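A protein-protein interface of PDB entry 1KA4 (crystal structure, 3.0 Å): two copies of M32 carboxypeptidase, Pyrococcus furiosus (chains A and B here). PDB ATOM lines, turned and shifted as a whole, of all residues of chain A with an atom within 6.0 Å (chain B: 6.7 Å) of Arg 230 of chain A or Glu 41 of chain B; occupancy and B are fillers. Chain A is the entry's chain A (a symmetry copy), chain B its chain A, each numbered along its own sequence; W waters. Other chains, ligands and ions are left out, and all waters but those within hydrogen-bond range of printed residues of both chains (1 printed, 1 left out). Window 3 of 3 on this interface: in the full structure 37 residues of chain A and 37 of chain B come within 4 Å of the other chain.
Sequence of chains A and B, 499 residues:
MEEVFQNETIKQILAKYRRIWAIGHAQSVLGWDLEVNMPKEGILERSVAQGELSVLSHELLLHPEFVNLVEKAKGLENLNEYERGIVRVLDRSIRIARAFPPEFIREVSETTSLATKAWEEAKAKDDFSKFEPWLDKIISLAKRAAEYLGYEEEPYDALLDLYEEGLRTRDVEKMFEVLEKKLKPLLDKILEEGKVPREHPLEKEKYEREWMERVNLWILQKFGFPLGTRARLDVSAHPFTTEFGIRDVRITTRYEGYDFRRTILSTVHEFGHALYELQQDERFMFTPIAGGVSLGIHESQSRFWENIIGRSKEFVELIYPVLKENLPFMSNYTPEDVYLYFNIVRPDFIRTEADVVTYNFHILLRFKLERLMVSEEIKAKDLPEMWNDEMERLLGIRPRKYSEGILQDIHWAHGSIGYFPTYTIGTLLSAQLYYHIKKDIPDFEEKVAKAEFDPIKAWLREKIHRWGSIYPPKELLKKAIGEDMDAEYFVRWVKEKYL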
ATOM      1  N   PRO A 226      -0.968  11.597  -9.853  1.00  0.00           N
ATOM      2  CA  PRO A 226      -1.634  10.723  -8.878  1.00  0.00           C
ATOM      3  C   PRO A 226      -0.761  10.024  -7.815  1.00  0.00           C
ATOM      4  O   PRO A 226      -0.648   8.793  -7.806  1.00  0.00           O
ATOM      5  CB  PRO A 226      -2.365   9.736  -9.773  1.00  0.00           C
ATOM      6  CG  PRO A 226      -1.392   9.530 -10.862  1.00  0.00           C
ATOM      7  CD  PRO A 226      -0.874  10.921 -11.160  1.00  0.00           C
ATOM      8  N   LEU A 227      -0.164  10.808  -6.916  1.00  0.00           N
ATOM      9  CA  LEU A 227       0.677  10.257  -5.867  1.00  0.00           C
ATOM     10  C   LEU A 227      -0.081   9.290  -4.951  1.00  0.00           C
ATOM     11  O   LEU A 227      -1.274   9.451  -4.723  1.00  0.00           O
ATOM     12  CB  LEU A 227       1.276  11.384  -5.028  1.00  0.00           C
ATOM     13  CG  LEU A 227       2.358  12.270  -5.641  1.00  0.00           C
ATOM     14  CD1 LEU A 227       3.428  11.409  -6.310  1.00  0.00           C
ATOM     15  CD2 LEU A 227       1.736  13.212  -6.651  1.00  0.00           C
ATOM     16  N   GLY A 228       0.620   8.286  -4.429  1.00  0.00           N
ATOM     17  CA  GLY A 228       0.000   7.323  -3.530  1.00  0.00           C
ATOM     18  C   GLY A 228      -1.110   6.458  -4.107  1.00  0.00           C
ATOM     19  O   GLY A 228      -1.496   5.444  -3.531  1.00  0.00           O
ATOM     20  N   THR A 229      -1.621   6.854  -5.260  1.00  0.00           N
ATOM     21  CA  THR A 229      -2.679   6.115  -5.905  1.00  0.00           C
ATOM     22  C   THR A 229      -2.198   5.328  -7.152  1.00  0.00           C
ATOM     23  O   THR A 229      -2.520   4.144  -7.315  1.00  0.00           O
ATOM     24  CB  THR A 229      -3.814   7.082  -6.281  1.00  0.00           C
ATOM     25  OG1 THR A 229      -4.994   6.337  -6.566  1.00  0.00           O
ATOM     26  CG2 THR A 229      -3.457   7.873  -7.520  1.00  0.00           C
ATOM     27  N   ARG A 230      -1.423   5.983  -8.016  1.00  0.00           N
ATOM     28  CA  ARG A 230      -0.923   5.353  -9.227  1.00  0.00           C
ATOM     29  C   ARG A 230       0.497   5.746  -9.532  1.00  0.00           C
ATOM     30  O   ARG A 230       1.058   5.301 -10.529  1.00  0.00           O
ATOM     31  CB  ARG A 230      -1.790   5.734 -10.417  1.00  0.00           C
ATOM     32  CG  ARG A 230      -3.075   4.972 -10.487  1.00  0.00           C
ATOM     33  CD  ARG A 230      -3.958   5.464 -11.605  1.00  0.00           C
ATOM     34  NE  ARG A 230      -4.551   4.324 -12.290  1.00  0.00           N
ATOM     35  CZ  ARG A 230      -5.784   4.301 -12.780  1.00  0.00           C
ATOM     36  NH1 ARG A 230      -6.560   5.367 -12.652  1.00  0.00           N
ATOM     37  NH2 ARG A 230      -6.233   3.215 -13.395  1.00  0.00           N
ATOM     38  N   ALA A 231       1.095   6.569  -8.685  1.00  0.00           N
ATOM     39  CA  ALA A 231       2.452   6.991  -8.960  1.00  0.00           C
ATOM     40  C   ALA A 231       3.245   7.349  -7.720  1.00  0.00           C
ATOM     41  O   ALA A 231       2.681   7.490  -6.640  1.00  0.00           O
ATOM     42  CB  ALA A 231       2.413   8.161  -9.895  1.00  0.00           C
ATOM     43  N   ARG A 232       4.555   7.498  -7.888  1.00  0.00           N
ATOM     44  CA  ARG A 232       5.438   7.871  -6.792  1.00  0.00           C
ATOM     45  C   ARG A 232       6.535   8.812  -7.290  1.00  0.00           C
ATOM     46  O   ARG A 232       6.822   8.883  -8.494  1.00  0.00           O
ATOM     47  CB  ARG A 232       6.134   6.643  -6.199  1.00  0.00           C
ATOM     48  CG  ARG A 232       5.259   5.565  -5.604  1.00  0.00           C
ATOM     49  CD  ARG A 232       6.157   4.557  -4.891  1.00  0.00           C
ATOM     50  NE  ARG A 232       7.091   5.254  -4.010  1.00  0.00           N
ATOM     51  CZ  ARG A 232       6.853   5.547  -2.734  1.00  0.00           C
ATOM     52  NH1 ARG A 232       5.702   5.185  -2.176  1.00  0.00           N
ATOM     53  NH2 ARG A 232       7.746   6.233  -2.029  1.00  0.00           N
ATOM     54  N   GLY A 245       3.345  -0.531 -14.302  1.00  0.00           N
ATOM     55  CA  GLY A 245       2.048  -0.794 -14.896  1.00  0.00           C
ATOM     56  C   GLY A 245       1.318   0.487 -15.263  1.00  0.00           C
ATOM     57  O   GLY A 245       1.804   1.595 -15.026  1.00  0.00           O
ATOM     58  N   ILE A 246       0.138   0.344 -15.844  1.00  0.00           N
ATOM     59  CA  ILE A 246      -0.634   1.516 -16.230  1.00  0.00           C
ATOM     60  C   ILE A 246      -1.111   2.225 -14.972  1.00  0.00           C
ATOM     61  O   ILE A 246      -1.346   3.429 -14.970  1.00  0.00           O
ATOM     62  CB  ILE A 246      -1.863   1.128 -17.075  1.00  0.00           C
ATOM     63  CG1 ILE A 246      -1.413   0.459 -18.380  1.00  0.00           C
ATOM     64  CG2 ILE A 246      -2.694   2.347 -17.362  1.00  0.00           C
ATOM     65  CD1 ILE A 246      -2.546  -0.070 -19.259  1.00  0.00           C
ATOM     66  N   ARG A 247      -1.248   1.467 -13.894  1.00  0.00           N
ATOM     67  CA  ARG A 247      -1.708   2.027 -12.643  1.00  0.00           C
ATOM     68  C   ARG A 247      -0.573   2.177 -11.633  1.00  0.00           C
ATOM     69  O   ARG A 247      -0.820   2.368 -10.432  1.00  0.00           O
ATOM     70  CB  ARG A 247      -2.801   1.140 -12.056  1.00  0.00           C
ATOM     71  CG  ARG A 247      -3.983   0.995 -12.957  1.00  0.00           C
ATOM     72  CD  ARG A 247      -5.071   0.138 -12.334  1.00  0.00           C
ATOM     73  NE  ARG A 247      -6.260   0.072 -13.184  1.00  0.00           N
ATOM     74  CZ  ARG A 247      -7.275  -0.769 -13.004  1.00  0.00           C
ATOM     75  NH1 ARG A 247      -7.255  -1.635 -11.989  1.00  0.00           N
ATOM     76  NH2 ARG A 247      -8.304  -0.753 -13.844  1.00  0.00           N
ATOM     77  N   ASP A 248       0.667   2.094 -12.110  1.00  0.00           N
ATOM     78  CA  ASP A 248       1.824   2.212 -11.231  1.00  0.00           C
ATOM     79  C   ASP A 248       2.983   2.736 -12.059  1.00  0.00           C
ATOM     80  O   ASP A 248       3.665   1.963 -12.726  1.00  0.00           O
ATOM     81  CB  ASP A 248       2.177   0.843 -10.642  1.00  0.00           C
ATOM     82  CG  ASP A 248       3.175   0.933  -9.487  1.00  0.00           C
ATOM     83  OD1 ASP A 248       3.763   2.004  -9.282  1.00  0.00           O
ATOM     84  OD2 ASP A 248       3.385  -0.077  -8.776  1.00  0.00           O
ATOM     85  N   VAL A 249       3.203   4.046 -12.033  1.00  0.00           N
ATOM     86  CA  VAL A 249       4.299   4.662 -12.784  1.00  0.00           C
ATOM     87  C   VAL A 249       5.082   5.500 -11.784  1.00  0.00           C
ATOM     88  O   VAL A 249       4.483   6.213 -10.988  1.00  0.00           O
ATOM     89  CB  VAL A 249       3.748   5.561 -13.936  1.00  0.00           C
ATOM     90  CG1 VAL A 249       4.894   6.231 -14.702  1.00  0.00           C
ATOM     91  CG2 VAL A 249       2.903   4.712 -14.889  1.00  0.00           C
ATOM     92  N   ARG A 250       6.408   5.432 -11.807  1.00  0.00           N
ATOM     93  CA  ARG A 250       7.176   6.181 -10.824  1.00  0.00           C
ATOM     94  C   ARG A 250       8.271   7.006 -11.432  1.00  0.00           C
ATOM     95  O   ARG A 250       8.869   6.612 -12.428  1.00  0.00           O
ATOM     96  CB  ARG A 250       7.770   5.211  -9.807  1.00  0.00           C
ATOM     97  CG  ARG A 250       6.748   4.189  -9.331  1.00  0.00           C
ATOM     98  CD  ARG A 250       7.299   3.225  -8.307  1.00  0.00           C
ATOM     99  NE  ARG A 250       6.294   2.218  -7.971  1.00  0.00           N
ATOM    100  CZ  ARG A 250       6.454   1.289  -7.034  1.00  0.00           C
ATOM    101  NH1 ARG A 250       7.581   1.226  -6.331  1.00  0.00           N
ATOM    102  NH2 ARG A 250       5.476   0.431  -6.789  1.00  0.00           N
ATOM    103  N   LEU A 278       1.046   6.770 -17.880  1.00  0.00           N
ATOM    104  CA  LEU A 278      -0.117   6.830 -17.021  1.00  0.00           C
ATOM    105  C   LEU A 278      -1.391   6.896 -17.838  1.00  0.00           C
ATOM    106  O   LEU A 278      -2.353   6.234 -17.505  1.00  0.00           O
ATOM    107  CB  LEU A 278      -0.011   8.059 -16.115  1.00  0.00           C
ATOM    108  CG  LEU A 278      -0.109   7.972 -14.577  1.00  0.00           C
ATOM    109  CD1 LEU A 278       0.478   6.689 -14.051  1.00  0.00           C
ATOM    110  CD2 LEU A 278       0.615   9.189 -13.968  1.00  0.00           C
ATOM    111  N   GLU A 282      -6.325   1.256 -20.753  1.00  0.00           N
ATOM    112  CA  GLU A 282      -6.400   0.036 -19.941  1.00  0.00           C
ATOM    113  C   GLU A 282      -6.939  -1.227 -20.603  1.00  0.00           C
ATOM    114  O   GLU A 282      -6.902  -2.297 -20.005  1.00  0.00           O
ATOM    115  CB  GLU A 282      -7.165   0.287 -18.641  1.00  0.00           C
ATOM    116  CG  GLU A 282      -6.513   1.336 -17.761  1.00  0.00           C
ATOM    117  CD  GLU A 282      -7.051   1.367 -16.347  1.00  0.00           C
ATOM    118  OE1 GLU A 282      -8.196   0.913 -16.112  1.00  0.00           O
ATOM    119  OE2 GLU A 282      -6.328   1.863 -15.468  1.00  0.00           O
ATOM    120  N   MET B  38       4.176   0.402  -3.092  1.00  0.00           N
ATOM    121  CA  MET B  38       3.158   0.390  -4.130  1.00  0.00           C
ATOM    122  C   MET B  38       1.928   1.251  -4.004  1.00  0.00           C
ATOM    123  O   MET B  38       1.193   1.138  -3.050  1.00  0.00           O
ATOM    124  CB  MET B  38       2.696  -1.040  -4.370  1.00  0.00           C
ATOM    125  CG  MET B  38       1.830  -1.182  -5.581  1.00  0.00           C
ATOM    126  SD  MET B  38       1.132  -2.788  -5.667  1.00  0.00           S
ATOM    127  CE  MET B  38      -0.209  -2.590  -4.568  1.00  0.00           C
ATOM    128  N   PRO B  39       1.693   2.145  -4.978  1.00  0.00           N
ATOM    129  CA  PRO B  39       0.486   2.982  -4.893  1.00  0.00           C
ATOM    130  C   PRO B  39      -0.746   2.048  -4.913  1.00  0.00           C
ATOM    131  O   PRO B  39      -0.832   1.124  -5.728  1.00  0.00           O
ATOM    132  CB  PRO B  39       0.577   3.899  -6.127  1.00  0.00           C
ATOM    133  CG  PRO B  39       1.771   3.416  -6.906  1.00  0.00           C
ATOM    134  CD  PRO B  39       2.655   2.682  -5.951  1.00  0.00           C
ATOM    135  N   LYS B  40      -1.673   2.298  -3.990  1.00  0.00           N
ATOM    136  CA  LYS B  40      -2.861   1.467  -3.843  1.00  0.00           C
ATOM    137  C   LYS B  40      -3.419   0.788  -5.091  1.00  0.00           C
ATOM    138  O   LYS B  40      -3.564  -0.415  -5.103  1.00  0.00           O
ATOM    139  CB  LYS B  40      -3.966   2.256  -3.129  1.00  0.00           C
ATOM    140  CG  LYS B  40      -3.582   2.776  -1.737  1.00  0.00           C
ATOM    141  CD  LYS B  40      -3.271   1.652  -0.728  1.00  0.00           C
ATOM    142  CE  LYS B  40      -2.959   2.230   0.667  1.00  0.00           C
ATOM    143  NZ  LYS B  40      -2.761   1.178   1.714  1.00  0.00           N
ATOM    144  N   GLU B  41      -3.700   1.554  -6.138  1.00  0.00           N
ATOM    145  CA  GLU B  41      -4.259   0.966  -7.366  1.00  0.00           C
ATOM    146  C   GLU B  41      -3.391   0.022  -8.213  1.00  0.00           C
ATOM    147  O   GLU B  41      -3.886  -0.582  -9.178  1.00  0.00           O
ATOM    148  CB  GLU B  41      -4.812   2.071  -8.275  1.00  0.00           C
ATOM    149  CG  GLU B  41      -6.102   2.696  -7.805  1.00  0.00           C
ATOM    150  CD  GLU B  41      -6.774   3.522  -8.898  1.00  0.00           C
ATOM    151  OE1 GLU B  41      -7.287   2.914  -9.877  1.00  0.00           O
ATOM    152  OE2 GLU B  41      -6.777   4.778  -8.789  1.00  0.00           O
ATOM    153  N   GLY B  42      -2.114  -0.105  -7.852  1.00  0.00           N
ATOM    154  CA  GLY B  42      -1.213  -0.970  -8.592  1.00  0.00           C
ATOM    155  C   GLY B  42      -1.324  -2.433  -8.209  1.00  0.00           C
ATOM    156  O   GLY B  42      -0.577  -3.288  -8.688  1.00  0.00           O
ATOM    157  N   ILE B  43      -2.282  -2.741  -7.356  1.00  0.00           N
ATOM    158  CA  ILE B  43      -2.474  -4.101  -6.893  1.00  0.00           C
ATOM    159  C   ILE B  43      -2.879  -5.117  -7.950  1.00  0.00           C
ATOM    160  O   ILE B  43      -2.388  -6.237  -7.929  1.00  0.00           O
ATOM    161  CB  ILE B  43      -3.499  -4.137  -5.754  1.00  0.00           C
ATOM    162  CG1 ILE B  43      -3.664  -5.565  -5.243  1.00  0.00           C
ATOM    163  CG2 ILE B  43      -4.794  -3.536  -6.217  1.00  0.00           C
ATOM    164  CD1 ILE B  43      -2.438  -6.109  -4.534  1.00  0.00           C
ATOM    165  N   LEU B  44      -3.764  -4.752  -8.873  1.00  0.00           N
ATOM    166  CA  LEU B  44      -4.194  -5.733  -9.872  1.00  0.00           C
ATOM    167  C   LEU B  44      -3.037  -6.243 -10.722  1.00  0.00           C
ATOM    168  O   LEU B  44      -2.868  -7.455 -10.909  1.00  0.00           O
ATOM    169  CB  LEU B  44      -5.283  -5.162 -10.798  1.00  0.00           C
ATOM    170  CG  LEU B  44      -5.656  -6.146 -11.924  1.00  0.00           C
ATOM    171  CD1 LEU B  44      -6.118  -7.476 -11.337  1.00  0.00           C
ATOM    172  CD2 LEU B  44      -6.716  -5.558 -12.793  1.00  0.00           C
ATOM    173  N   GLU B  45      -2.248  -5.305 -11.239  1.00  0.00           N
ATOM    174  CA  GLU B  45      -1.105  -5.638 -12.072  1.00  0.00           C
ATOM    175  C   GLU B  45      -0.004  -6.323 -11.259  1.00  0.00           C
ATOM    176  O   GLU B  45       0.678  -7.220 -11.755  1.00  0.00           O
ATOM    177  CB  GLU B  45      -0.610  -4.370 -12.768  1.00  0.00           C
ATOM    178  CG  GLU B  45      -1.585  -3.905 -13.849  1.00  0.00           C
ATOM    179  CD  GLU B  45      -1.336  -2.477 -14.319  1.00  0.00           C
ATOM    180  OE1 GLU B  45      -1.407  -1.577 -13.450  1.00  0.00           O
ATOM    181  OE2 GLU B  45      -1.083  -2.251 -15.537  1.00  0.00           O
HETATM  182  O   HOH W   1       2.335  -2.490  -9.334  1.00  0.00           O
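OE1 of Glu 45 of chain B lies within hydrogen-bond range of N of Arg 247 of chain A (3.1 Å). O of Gly 228 of chain A is in hydrogen-bond range of N of Lys 40 of chain B. The backbone NH (N) of Glu 41 of chain B lies within hydrogen-bond range of the backbone carbonyl oxygen (O) of Thr 229 of chain A. The side-chain carboxylate of Glu 41 of chain B is in salt-bridge range of the guanidinium group of Arg 230 of chain A (3.7 Å). N of Ile 246 of chain A lies within hydrogen-bond range of OE2 of Glu 45 of chain B (2.9 Å).
The side-chain carboxylate (OE2) of Glu 282 of chain A is in salt-bridge range of the guanidinium group (NH2) of Arg 230 of chain A, 2.5 Å away. The backbone carbonyl oxygen (O) of Arg 230 of chain A sits at hydrogen-bond distance from the backbone NH (N) of Val 249 of chain A (2.9 Å). The backbone NH (N) of Arg 232 of chain A sits at hydrogen-bond distance from the backbone carbonyl oxygen (O) of Val 249 of chain A (3.4 Å). The guanidinium group (NE) of Arg 250 of chain A is in salt-bridge range of the side-chain carboxylate (OD1) of Asp 248 of chain A (2.9 Å). The guanidinium group (NH2) of Arg 247 of chain A lies within salt-bridge range of the side-chain carboxylate (OE1) of Glu 282 of chain A, at 2.8 Å. O of Pro 226 of chain A sits at hydrogen-bond distance from N of Ala 231 of chain A (3.0 Å).
Among the printed residues, pairs that only touch across the chains: Gly 228 of chain A with Pro 39 of chain B (3.4 Å), Thr 229 of chain A with Pro 39 of chain B (3.3 Å), Thr 229 of chain A with Lys 40 of chain B (3.9 Å), Arg 230 of chain A with Pro 39 of chain B (3.5 Å), Ala 231 of chain A with Pro 39 of chain B (3.7 Å), Arg 232 of chain A with Pro 39 of chain B (3.9 Å), Gly 245 of chain A with Glu 45 of chain B (3.5 Å), Arg 247 of chain A with Glu 41 of chain B (3.4 Å), Arg 247 of chain A with Gly 42 of chain B (3.8 Å), Asp 248 of chain A with Met 38 of chain B (3.7 Å), Asp 248 of chain A with Pro 39 of chain B (3.4 Å), Arg 250 of chain A with Met 38 of chain B (3.5 Å) and Arg 250 of chain A with Pro 39 of chain B (3.7 Å).
Arg 230 of chain A touches just these residues of chain B: Pro 39 (3.5 Å) and Glu 41 (3.6 Å). Glu 41 of chain B touches just these residues of chain A: Thr 229, Arg 230 and Arg 247. Printed residues of chain A within 4 Å of Gly 42 of chain B: Arg 247 (3.8 Å). Printed residues of chain B within 4 Å of Arg 247 of chain A: Glu 41 (3.4 Å), Gly 42 (3.8 Å) and Glu 45 (3.1 Å). Of the printed residues of chain A, Lys 40 of chain B touches Gly 228 and Thr 229. Printed residues of chain B within 4 Å of Thr 229 of chain A: Pro 39 (3.3 Å), Lys 40 (3.9 Å) and Glu 41 (3.1 Å). The nearest residue of chain A that does not touch Glu 41 of chain B is Gly 228 of chain A (5.2 Å).
Of the 8 printed residues of chain B, 6 touch a printed residue of chain A. Printed residues of chain A that touch a printed residue of chain B: Gly 228, Thr 229, Arg 230, Ala 231, Arg 232, Gly 245, Ile 246, Arg 247, Asp 248 and Arg 250. Among the printed residues, 18 pairs touch across the chains. Among the printed residues, Asp or Glu carboxylates within 4 Å of a Lys or Arg side-chain nitrogen of the other chain: Arg 230 of chain A with Glu 41 of chain B.
No position is printed for both chains.
Water W1 bridges OD2 of Asp 248 of chain A and O of Gly 42 of chain B.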
